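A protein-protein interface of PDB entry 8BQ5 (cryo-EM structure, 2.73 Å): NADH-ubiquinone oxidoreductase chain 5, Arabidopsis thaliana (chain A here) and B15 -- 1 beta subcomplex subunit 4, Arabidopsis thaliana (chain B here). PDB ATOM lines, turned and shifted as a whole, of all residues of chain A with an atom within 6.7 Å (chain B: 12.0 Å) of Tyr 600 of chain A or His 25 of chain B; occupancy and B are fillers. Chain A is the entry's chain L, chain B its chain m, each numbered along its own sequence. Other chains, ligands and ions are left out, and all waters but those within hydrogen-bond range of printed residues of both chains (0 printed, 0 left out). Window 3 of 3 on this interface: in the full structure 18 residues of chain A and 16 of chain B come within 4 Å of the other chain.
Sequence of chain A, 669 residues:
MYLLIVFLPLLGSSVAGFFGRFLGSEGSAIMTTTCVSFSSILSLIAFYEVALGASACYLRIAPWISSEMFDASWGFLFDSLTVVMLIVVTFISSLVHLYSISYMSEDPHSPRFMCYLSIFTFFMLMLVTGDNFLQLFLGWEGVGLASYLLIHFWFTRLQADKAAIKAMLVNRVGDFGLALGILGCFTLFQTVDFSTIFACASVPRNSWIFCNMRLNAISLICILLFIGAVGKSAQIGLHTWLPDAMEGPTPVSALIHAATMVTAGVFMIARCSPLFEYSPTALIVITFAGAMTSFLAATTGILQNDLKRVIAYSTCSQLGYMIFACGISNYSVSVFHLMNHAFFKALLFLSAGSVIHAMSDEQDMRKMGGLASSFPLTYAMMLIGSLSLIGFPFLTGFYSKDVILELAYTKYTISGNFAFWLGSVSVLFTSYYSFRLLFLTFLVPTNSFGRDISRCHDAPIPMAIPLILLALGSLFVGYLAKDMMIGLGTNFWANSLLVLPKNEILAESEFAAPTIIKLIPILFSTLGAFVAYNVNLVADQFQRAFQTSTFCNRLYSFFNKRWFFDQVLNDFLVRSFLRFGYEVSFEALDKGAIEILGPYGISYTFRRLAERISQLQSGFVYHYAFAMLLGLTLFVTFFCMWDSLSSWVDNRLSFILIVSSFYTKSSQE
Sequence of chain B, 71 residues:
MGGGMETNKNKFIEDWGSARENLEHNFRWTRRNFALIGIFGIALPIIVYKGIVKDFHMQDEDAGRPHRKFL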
ATOM      1  N   LYS A 591      -9.595  32.590  14.138  1.00  0.00           N
ATOM      2  CA  LYS A 591      -8.535  31.712  13.666  1.00  0.00           C
ATOM      3  C   LYS A 591      -7.618  31.247  14.786  1.00  0.00           C
ATOM      4  O   LYS A 591      -6.605  30.598  14.508  1.00  0.00           O
ATOM      5  CB  LYS A 591      -7.711  32.408  12.581  1.00  0.00           C
ATOM      6  CG  LYS A 591      -8.477  32.656  11.297  1.00  0.00           C
ATOM      7  CD  LYS A 591      -9.188  31.396  10.835  1.00  0.00           C
ATOM      8  CE  LYS A 591      -8.863  31.073   9.389  1.00  0.00           C
ATOM      9  NZ  LYS A 591      -9.100  29.634   9.089  1.00  0.00           N
ATOM     10  N   GLY A 592      -7.940  31.563  16.037  1.00  0.00           N
ATOM     11  CA  GLY A 592      -7.099  31.181  17.153  1.00  0.00           C
ATOM     12  C   GLY A 592      -7.737  30.185  18.097  1.00  0.00           C
ATOM     13  O   GLY A 592      -7.807  28.990  17.800  1.00  0.00           O
ATOM     14  N   ILE A 594     -10.823  29.608  19.052  1.00  0.00           N
ATOM     15  CA  ILE A 594     -11.999  28.890  18.575  1.00  0.00           C
ATOM     16  C   ILE A 594     -11.591  27.791  17.599  1.00  0.00           C
ATOM     17  O   ILE A 594     -12.214  26.723  17.549  1.00  0.00           O
ATOM     18  CB  ILE A 594     -13.010  29.876  17.962  1.00  0.00           C
ATOM     19  CG1 ILE A 594     -13.379  30.947  18.990  1.00  0.00           C
ATOM     20  CG2 ILE A 594     -14.257  29.150  17.495  1.00  0.00           C
ATOM     21  CD1 ILE A 594     -14.286  32.028  18.455  1.00  0.00           C
ATOM     22  N   GLU A 595     -10.542  28.031  16.810  1.00  0.00           N
ATOM     23  CA  GLU A 595     -10.010  26.973  15.957  1.00  0.00           C
ATOM     24  C   GLU A 595      -9.329  25.881  16.778  1.00  0.00           C
ATOM     25  O   GLU A 595      -9.611  24.693  16.589  1.00  0.00           O
ATOM     26  CB  GLU A 595      -9.040  27.565  14.935  1.00  0.00           C
ATOM     27  CG  GLU A 595      -9.661  27.935  13.588  1.00  0.00           C
ATOM     28  CD  GLU A 595     -10.203  26.741  12.818  1.00  0.00           C
ATOM     29  OE1 GLU A 595     -11.217  26.150  13.242  1.00  0.00           O
ATOM     30  OE2 GLU A 595      -9.608  26.394  11.777  1.00  0.00           O
ATOM     31  N   ILE A 596      -8.440  26.261  17.702  1.00  0.00           N
ATOM     32  CA  ILE A 596      -7.700  25.260  18.467  1.00  0.00           C
ATOM     33  C   ILE A 596      -8.639  24.498  19.396  1.00  0.00           C
ATOM     34  O   ILE A 596      -8.587  23.266  19.478  1.00  0.00           O
ATOM     35  CB  ILE A 596      -6.533  25.913  19.234  1.00  0.00           C
ATOM     36  CG1 ILE A 596      -5.234  25.812  18.431  1.00  0.00           C
ATOM     37  CG2 ILE A 596      -6.318  25.236  20.577  1.00  0.00           C
ATOM     38  CD1 ILE A 596      -5.331  26.322  17.010  1.00  0.00           C
ATOM     39  N   LEU A 597      -9.513  25.210  20.100  1.00  0.00           N
ATOM     40  CA  LEU A 597     -10.607  24.569  20.829  1.00  0.00           C
ATOM     41  C   LEU A 597     -11.804  24.348  19.913  1.00  0.00           C
ATOM     42  O   LEU A 597     -12.936  24.715  20.225  1.00  0.00           O
ATOM     43  CB  LEU A 597     -10.998  25.403  22.044  1.00  0.00           C
ATOM     44  CG  LEU A 597     -10.084  25.406  23.269  1.00  0.00           C
ATOM     45  CD1 LEU A 597      -8.963  26.422  23.126  1.00  0.00           C
ATOM     46  CD2 LEU A 597     -10.907  25.688  24.513  1.00  0.00           C
ATOM     47  N   GLY A 598     -11.550  23.734  18.763  1.00  0.00           N
ATOM     48  CA  GLY A 598     -12.573  23.527  17.772  1.00  0.00           C
ATOM     49  C   GLY A 598     -12.107  22.615  16.659  1.00  0.00           C
ATOM     50  O   GLY A 598     -11.356  21.662  16.881  1.00  0.00           O
ATOM     51  N   PRO A 599     -12.529  22.912  15.429  1.00  0.00           N
ATOM     52  CA  PRO A 599     -12.288  21.966  14.324  1.00  0.00           C
ATOM     53  C   PRO A 599     -10.820  21.669  14.066  1.00  0.00           C
ATOM     54  O   PRO A 599     -10.489  20.540  13.686  1.00  0.00           O
ATOM     55  CB  PRO A 599     -12.950  22.642  13.114  1.00  0.00           C
ATOM     56  CG  PRO A 599     -13.584  23.887  13.607  1.00  0.00           C
ATOM     57  CD  PRO A 599     -13.117  24.184  14.984  1.00  0.00           C
ATOM     58  N   TYR A 600      -9.927  22.645  14.241  1.00  0.00           N
ATOM     59  CA  TYR A 600      -8.506  22.362  14.069  1.00  0.00           C
ATOM     60  C   TYR A 600      -7.994  21.430  15.159  1.00  0.00           C
ATOM     61  O   TYR A 600      -7.344  20.418  14.872  1.00  0.00           O
ATOM     62  CB  TYR A 600      -7.701  23.659  14.063  1.00  0.00           C
ATOM     63  CG  TYR A 600      -6.259  23.458  13.661  1.00  0.00           C
ATOM     64  CD1 TYR A 600      -5.926  23.077  12.370  1.00  0.00           C
ATOM     65  CD2 TYR A 600      -5.231  23.628  14.579  1.00  0.00           C
ATOM     66  CE1 TYR A 600      -4.613  22.887  11.997  1.00  0.00           C
ATOM     67  CE2 TYR A 600      -3.911  23.438  14.216  1.00  0.00           C
ATOM     68  CZ  TYR A 600      -3.609  23.067  12.922  1.00  0.00           C
ATOM     69  OH  TYR A 600      -2.301  22.874  12.548  1.00  0.00           O
ATOM     70  N   GLY A 601      -8.266  21.768  16.418  1.00  0.00           N
ATOM     71  CA  GLY A 601      -7.811  20.932  17.516  1.00  0.00           C
ATOM     72  C   GLY A 601      -8.533  19.603  17.586  1.00  0.00           C
ATOM     73  O   GLY A 601      -7.928  18.577  17.901  1.00  0.00           O
ATOM     74  N   ILE A 602      -9.841  19.605  17.313  1.00  0.00           N
ATOM     75  CA  ILE A 602     -10.625  18.374  17.377  1.00  0.00           C
ATOM     76  C   ILE A 602     -10.159  17.384  16.318  1.00  0.00           C
ATOM     77  O   ILE A 602     -10.052  16.179  16.577  1.00  0.00           O
ATOM     78  CB  ILE A 602     -12.126  18.691  17.240  1.00  0.00           C
ATOM     79  CG1 ILE A 602     -12.705  19.108  18.592  1.00  0.00           C
ATOM     80  CG2 ILE A 602     -12.885  17.507  16.657  1.00  0.00           C
ATOM     81  CD1 ILE A 602     -13.838  20.097  18.492  1.00  0.00           C
ATOM     82  N   SER A 603      -9.878  17.873  15.110  1.00  0.00           N
ATOM     83  CA  SER A 603      -9.406  16.991  14.047  1.00  0.00           C
ATOM     84  C   SER A 603      -8.067  16.357  14.404  1.00  0.00           C
ATOM     85  O   SER A 603      -7.854  15.161  14.167  1.00  0.00           O
ATOM     86  CB  SER A 603      -9.306  17.770  12.736  1.00  0.00           C
ATOM     87  OG  SER A 603      -8.013  18.317  12.559  1.00  0.00           O
ATOM     88  N   TYR A 604      -7.159  17.140  14.990  1.00  0.00           N
ATOM     89  CA  TYR A 604      -5.830  16.638  15.328  1.00  0.00           C
ATOM     90  C   TYR A 604      -5.902  15.512  16.354  1.00  0.00           C
ATOM     91  O   TYR A 604      -5.297  14.446  16.171  1.00  0.00           O
ATOM     92  CB  TYR A 604      -4.963  17.800  15.833  1.00  0.00           C
ATOM     93  CG  TYR A 604      -3.748  17.416  16.658  1.00  0.00           C
ATOM     94  CD1 TYR A 604      -3.854  17.148  18.020  1.00  0.00           C
ATOM     95  CD2 TYR A 604      -2.493  17.327  16.072  1.00  0.00           C
ATOM     96  CE1 TYR A 604      -2.749  16.799  18.768  1.00  0.00           C
ATOM     97  CE2 TYR A 604      -1.381  16.979  16.815  1.00  0.00           C
ATOM     98  CZ  TYR A 604      -1.515  16.715  18.161  1.00  0.00           C
ATOM     99  OH  TYR A 604      -0.411  16.370  18.904  1.00  0.00           O
ATOM    100  N   THR A 605      -6.643  15.729  17.444  1.00  0.00           N
ATOM    101  CA  THR A 605      -6.666  14.738  18.514  1.00  0.00           C
ATOM    102  C   THR A 605      -7.374  13.467  18.072  1.00  0.00           C
ATOM    103  O   THR A 605      -6.968  12.363  18.447  1.00  0.00           O
ATOM    104  CB  THR A 605      -7.330  15.306  19.769  1.00  0.00           C
ATOM    105  OG1 THR A 605      -7.642  14.236  20.668  1.00  0.00           O
ATOM    106  CG2 THR A 605      -8.613  16.027  19.422  1.00  0.00           C
ATOM    107  N   ASP B  15       0.355  34.813  -2.445  1.00  0.00           N
ATOM    108  CA  ASP B  15       0.947  34.366  -1.187  1.00  0.00           C
ATOM    109  C   ASP B  15       0.365  35.142  -0.012  1.00  0.00           C
ATOM    110  O   ASP B  15       0.073  34.565   1.042  1.00  0.00           O
ATOM    111  CB  ASP B  15       2.468  34.513  -1.229  1.00  0.00           C
ATOM    112  CG  ASP B  15       3.150  33.342  -1.907  1.00  0.00           C
ATOM    113  OD1 ASP B  15       4.271  32.984  -1.489  1.00  0.00           O
ATOM    114  OD2 ASP B  15       2.568  32.777  -2.857  1.00  0.00           O
ATOM    115  N   GLY B  17      -2.622  36.325  -0.017  1.00  0.00           N
ATOM    116  CA  GLY B  17      -3.975  35.817   0.138  1.00  0.00           C
ATOM    117  C   GLY B  17      -4.024  34.475   0.841  1.00  0.00           C
ATOM    118  O   GLY B  17      -4.889  34.235   1.687  1.00  0.00           O
ATOM    119  N   SER B  18      -3.097  33.578   0.498  1.00  0.00           N
ATOM    120  CA  SER B  18      -3.111  32.242   1.083  1.00  0.00           C
ATOM    121  C   SER B  18      -2.603  32.241   2.517  1.00  0.00           C
ATOM    122  O   SER B  18      -2.981  31.369   3.306  1.00  0.00           O
ATOM    123  CB  SER B  18      -2.288  31.283   0.226  1.00  0.00           C
ATOM    124  OG  SER B  18      -2.931  31.042  -1.014  1.00  0.00           O
ATOM    125  N   ALA B  19      -1.744  33.199   2.873  1.00  0.00           N
ATOM    126  CA  ALA B  19      -1.307  33.307   4.260  1.00  0.00           C
ATOM    127  C   ALA B  19      -2.490  33.553   5.183  1.00  0.00           C
ATOM    128  O   ALA B  19      -2.589  32.949   6.256  1.00  0.00           O
ATOM    129  CB  ALA B  19      -0.274  34.424   4.404  1.00  0.00           C
ATOM    130  N   ARG B  20      -3.410  34.426   4.766  1.00  0.00           N
ATOM    131  CA  ARG B  20      -4.564  34.761   5.594  1.00  0.00           C
ATOM    132  C   ARG B  20      -5.448  33.544   5.848  1.00  0.00           C
ATOM    133  O   ARG B  20      -5.953  33.357   6.960  1.00  0.00           O
ATOM    134  CB  ARG B  20      -5.364  35.881   4.930  1.00  0.00           C
ATOM    135  CG  ARG B  20      -6.577  36.310   5.721  1.00  0.00           C
ATOM    136  CD  ARG B  20      -6.196  37.213   6.881  1.00  0.00           C
ATOM    137  NE  ARG B  20      -5.208  38.226   6.526  1.00  0.00           N
ATOM    138  CZ  ARG B  20      -5.514  39.466   6.169  1.00  0.00           C
ATOM    139  NH1 ARG B  20      -6.770  39.873   6.094  1.00  0.00           N
ATOM    140  NH2 ARG B  20      -4.535  40.322   5.889  1.00  0.00           N
ATOM    141  N   GLU B  21      -5.653  32.707   4.829  1.00  0.00           N
ATOM    142  CA  GLU B  21      -6.556  31.568   4.952  1.00  0.00           C
ATOM    143  C   GLU B  21      -6.029  30.476   5.872  1.00  0.00           C
ATOM    144  O   GLU B  21      -6.807  29.604   6.270  1.00  0.00           O
ATOM    145  CB  GLU B  21      -6.836  30.962   3.577  1.00  0.00           C
ATOM    146  CG  GLU B  21      -6.822  31.961   2.449  1.00  0.00           C
ATOM    147  CD  GLU B  21      -7.662  31.520   1.276  1.00  0.00           C
ATOM    148  OE1 GLU B  21      -7.090  31.283   0.191  1.00  0.00           O
ATOM    149  OE2 GLU B  21      -8.895  31.410   1.437  1.00  0.00           O
ATOM    150  N   ASN B  22      -4.744  30.496   6.212  1.00  0.00           N
ATOM    151  CA  ASN B  22      -4.119  29.445   7.003  1.00  0.00           C
ATOM    152  C   ASN B  22      -3.536  30.016   8.288  1.00  0.00           C
ATOM    153  O   ASN B  22      -2.423  29.679   8.697  1.00  0.00           O
ATOM    154  CB  ASN B  22      -3.050  28.727   6.183  1.00  0.00           C
ATOM    155  CG  ASN B  22      -3.644  27.904   5.055  1.00  0.00           C
ATOM    156  OD1 ASN B  22      -3.598  28.300   3.890  1.00  0.00           O
ATOM    157  ND2 ASN B  22      -4.207  26.752   5.397  1.00  0.00           N
ATOM    158  N   LEU B  23      -4.297  30.892   8.950  1.00  0.00           N
ATOM    159  CA  LEU B  23      -3.798  31.561  10.146  1.00  0.00           C
ATOM    160  C   LEU B  23      -3.802  30.646  11.363  1.00  0.00           C
ATOM    161  O   LEU B  23      -2.982  30.824  12.270  1.00  0.00           O
ATOM    162  CB  LEU B  23      -4.626  32.811  10.432  1.00  0.00           C
ATOM    163  CG  LEU B  23      -3.830  34.050  10.841  1.00  0.00           C
ATOM    164  CD1 LEU B  23      -2.690  34.300   9.869  1.00  0.00           C
ATOM    165  CD2 LEU B  23      -4.740  35.261  10.937  1.00  0.00           C
ATOM    166  N   GLU B  24      -4.715  29.674  11.413  1.00  0.00           N
ATOM    167  CA  GLU B  24      -4.780  28.781  12.564  1.00  0.00           C
ATOM    168  C   GLU B  24      -3.555  27.881  12.667  1.00  0.00           C
ATOM    169  O   GLU B  24      -3.310  27.309  13.735  1.00  0.00           O
ATOM    170  CB  GLU B  24      -6.050  27.929  12.504  1.00  0.00           C
ATOM    171  CG  GLU B  24      -6.095  26.958  11.339  1.00  0.00           C
ATOM    172  CD  GLU B  24      -6.582  27.597  10.055  1.00  0.00           C
ATOM    173  OE1 GLU B  24      -5.942  28.559   9.586  1.00  0.00           O
ATOM    174  OE2 GLU B  24      -7.602  27.127   9.509  1.00  0.00           O
ATOM    175  N   HIS B  25      -2.781  27.739  11.589  1.00  0.00           N
ATOM    176  CA  HIS B  25      -1.543  26.973  11.671  1.00  0.00           C
ATOM    177  C   HIS B  25      -0.451  27.706  12.436  1.00  0.00           C
ATOM    178  O   HIS B  25       0.545  27.077  12.808  1.00  0.00           O
ATOM    179  CB  HIS B  25      -1.028  26.626  10.272  1.00  0.00           C
ATOM    180  CG  HIS B  25      -1.991  25.831   9.446  1.00  0.00           C
ATOM    181  ND1 HIS B  25      -3.206  25.395   9.928  1.00  0.00           N
ATOM    182  CD2 HIS B  25      -1.918  25.399   8.166  1.00  0.00           C
ATOM    183  CE1 HIS B  25      -3.840  24.728   8.981  1.00  0.00           C
ATOM    184  NE2 HIS B  25      -3.079  24.715   7.902  1.00  0.00           N
ATOM    185  N   ASN B  26      -0.563  29.026  12.563  1.00  0.00           N
ATOM    186  CA  ASN B  26       0.536  29.792  13.203  1.00  0.00           C
ATOM    187  C   ASN B  26       0.177  30.123  14.651  1.00  0.00           C
ATOM    188  O   ASN B  26       0.987  30.803  15.299  1.00  0.00           O
ATOM    189  CB  ASN B  26       0.834  31.096  12.460  1.00  0.00           C
ATOM    190  CG  ASN B  26       1.025  30.912  10.971  1.00  0.00           C
ATOM    191  OD1 ASN B  26       0.054  30.781  10.230  1.00  0.00           O
ATOM    192  ND2 ASN B  26       2.271  30.912  10.526  1.00  0.00           N
ATOM    193  N   PHE B  27      -0.969  29.653  15.147  1.00  0.00           N
ATOM    194  CA  PHE B  27      -1.401  30.071  16.509  1.00  0.00           C
ATOM    195  C   PHE B  27      -0.545  29.390  17.575  1.00  0.00           C
ATOM    196  O   PHE B  27      -0.589  28.150  17.685  1.00  0.00           O
ATOM    197  CB  PHE B  27      -2.898  29.831  16.737  1.00  0.00           C
ATOM    198  CG  PHE B  27      -3.409  30.235  18.097  1.00  0.00           C
ATOM    199  CD1 PHE B  27      -3.777  31.545  18.357  1.00  0.00           C
ATOM    200  CD2 PHE B  27      -3.531  29.306  19.118  1.00  0.00           C
ATOM    201  CE1 PHE B  27      -4.250  31.918  19.605  1.00  0.00           C
ATOM    202  CE2 PHE B  27      -4.002  29.679  20.366  1.00  0.00           C
ATOM    203  CZ  PHE B  27      -4.360  30.983  20.608  1.00  0.00           C
ATOM    204  N   ARG B  28       0.192  30.195  18.344  1.00  0.00           N
ATOM    205  CA  ARG B  28       1.023  29.669  19.452  1.00  0.00           C
ATOM    206  C   ARG B  28       0.548  30.362  20.729  1.00  0.00           C
ATOM    207  O   ARG B  28       0.350  31.587  20.680  1.00  0.00           O
ATOM    208  CB  ARG B  28       2.497  30.003  19.217  1.00  0.00           C
ATOM    209  CG  ARG B  28       3.097  29.379  17.967  1.00  0.00           C
ATOM    210  CD  ARG B  28       3.081  27.865  18.022  1.00  0.00           C
ATOM    211  NE  ARG B  28       3.718  27.301  16.840  1.00  0.00           N
ATOM    212  CZ  ARG B  28       3.086  26.971  15.720  1.00  0.00           C
ATOM    213  NH1 ARG B  28       1.778  27.138  15.618  1.00  0.00           N
ATOM    214  NH2 ARG B  28       3.767  26.472  14.705  1.00  0.00           N
ATOM    215  N   TRP B  29       0.354  29.608  21.808  1.00  0.00           N
ATOM    216  CA  TRP B  29      -0.153  30.195  23.077  1.00  0.00           C
ATOM    217  C   TRP B  29       0.918  31.100  23.673  1.00  0.00           C
ATOM    218  O   TRP B  29       1.598  30.678  24.625  1.00  0.00           O
ATOM    219  CB  TRP B  29      -0.574  29.112  24.068  1.00  0.00           C
ATOM    220  CG  TRP B  29      -1.810  28.371  23.669  1.00  0.00           C
ATOM    221  CD1 TRP B  29      -1.882  27.178  23.010  1.00  0.00           C
ATOM    222  CD2 TRP B  29      -3.169  28.776  23.909  1.00  0.00           C
ATOM    223  NE1 TRP B  29      -3.188  26.813  22.826  1.00  0.00           N
ATOM    224  CE2 TRP B  29      -4.000  27.773  23.368  1.00  0.00           C
ATOM    225  CE3 TRP B  29      -3.760  29.883  24.528  1.00  0.00           C
ATOM    226  CZ2 TRP B  29      -5.390  27.851  23.426  1.00  0.00           C
ATOM    227  CZ3 TRP B  29      -5.133  29.955  24.589  1.00  0.00           C
ATOM    228  CH2 TRP B  29      -5.934  28.954  24.043  1.00  0.00           C
ATOM    229  N   THR B  30       1.040  32.311  23.140  1.00  0.00           N
ATOM    230  CA  THR B  30       2.021  33.283  23.671  1.00  0.00           C
ATOM    231  C   THR B  30       1.390  34.031  24.842  1.00  0.00           C
ATOM    232  O   THR B  30       0.198  33.803  25.115  1.00  0.00           O
ATOM    233  CB  THR B  30       2.450  34.279  22.591  1.00  0.00           C
ATOM    234  OG1 THR B  30       1.317  35.062  22.213  1.00  0.00           O
ATOM    235  CG2 THR B  30       3.033  33.607  21.367  1.00  0.00           C
ATOM    236  N   ASN B  33      -1.418  36.185  23.467  1.00  0.00           N
ATOM    237  CA  ASN B  33      -2.677  35.460  23.162  1.00  0.00           C
ATOM    238  C   ASN B  33      -3.409  35.143  24.468  1.00  0.00           C
ATOM    239  O   ASN B  33      -4.631  35.280  24.487  1.00  0.00           O
ATOM    240  CB  ASN B  33      -2.399  34.242  22.273  1.00  0.00           C
ATOM    241  CG  ASN B  33      -2.022  34.646  20.863  1.00  0.00           C
ATOM    242  OD1 ASN B  33      -2.221  35.793  20.469  1.00  0.00           O
ATOM    243  ND2 ASN B  33      -1.482  33.717  20.095  1.00  0.00           N
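The side-chain amino group of Lys 591 of chain A is in salt-bridge range of the side-chain carboxylate of Glu 24 of chain B.
The side-chain carboxylate (OE2) of Glu 595 of chain A lies close to the side-chain carboxylate (OE2) of Glu 24 of chain B, at 3.1 Å.
The side-chain amide nitrogen of Asn 22 of chain B lies within hydrogen-bond range of a ring nitrogen (NE2) of His 25 of chain B (3.4 Å).
The backbone carbonyl oxygen (O) of Glu 595 of chain A is in hydrogen-bond range of the backbone NH (N) of Tyr 600 of chain A, 3.1 Å away.
O of Glu 595 of chain A sits at hydrogen-bond distance from N of Gly 601 of chain A (3.2 Å).
The backbone carbonyl oxygen (O) of Ile 596 of chain A lies close to the backbone NH (N) of Gly 601 of chain A (3.4 Å).
The backbone carbonyl oxygen of His 25 of chain B sits at hydrogen-bond distance from the guanidinium group of Arg 28 of chain B.
The side-chain hydroxyl (OG) of Ser 603 of chain A sits at hydrogen-bond distance from the backbone carbonyl oxygen (O) of Tyr 600 of chain A (3.2 Å).
Among the printed residues, pairs that only touch across the chains: Tyr 600 of chain A with His 25 of chain B, Gly 592 of chain A with Phe 27 of chain B, Lys 591 of chain A with Glu 21 of chain B, Lys 591 of chain A with Leu 23 of chain B, Leu 597 of chain A with Trp 29 of chain B, Tyr 600 of chain A with Glu 24 of chain B, Ile 596 of chain A with Phe 27 of chain B, Ile 596 of chain A with Glu 24 of chain B and Ile 596 of chain A with Trp 29 of chain B.
Printed residues of chain B within 4 Å of Lys 591 of chain A: Glu 21 (3.6 Å), Leu 23 (3.8 Å) and Glu 24 (3.0 Å).
Of chain B, only Phe 27 comes within 4 Å of Gly 592 of chain A.
Of chain B, only Glu 24 comes within 4 Å of Glu 595 of chain A.
Tyr 600 of chain A touches just these residues of chain B: Glu 24 and His 25.
No residue of chain B comes within 4 Å of Gly 601 of chain A.
Asn 22 of chain B touches none of the printed residues of chain A.
Printed residues of chain A within 4 Å of Glu 24 of chain B: Lys 591 (3.0 Å), Glu 595 (3.1 Å), Ile 596 (3.97 Å) and Tyr 600 (3.9 Å).
Of chain A, only Tyr 600 comes within 4 Å of His 25 of chain B.
Printed residues of chain A within 4 Å of Trp 29 of chain B: Ile 596 (3.98 Å) and Leu 597 (3.9 Å).
The nearest residue of chain B that does not touch Tyr 600 of chain A is Asn 26 of chain B (6.4 Å).
The nearest residue of chain A that does not touch His 25 of chain B is Lys 591 of chain A (5.6 Å).
The nearest printed residue of chain A that does not touch Phe 27 of chain B is Lys 591 of chain A (4.4 Å).
Hydrophobic or aromatic side chains of chain A within 4 Å of the printed part of chain B: Ile 596, Leu 597 and Tyr 600.
Of the 16 printed residues of chain B, 6 touch a printed residue of chain A.
Printed residues of chain B that touch a printed residue of chain A: Glu 21, Leu 23, Glu 24, His 25, Phe 27 and Trp 29.
Among the printed residues, 11 pairs touch across the chains.
Among the printed residues, Asp or Glu carboxylates within 4 Å of a Lys or Arg side-chain nitrogen of the other chain: Lys 591 of chain A with Glu 24 of chain B.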
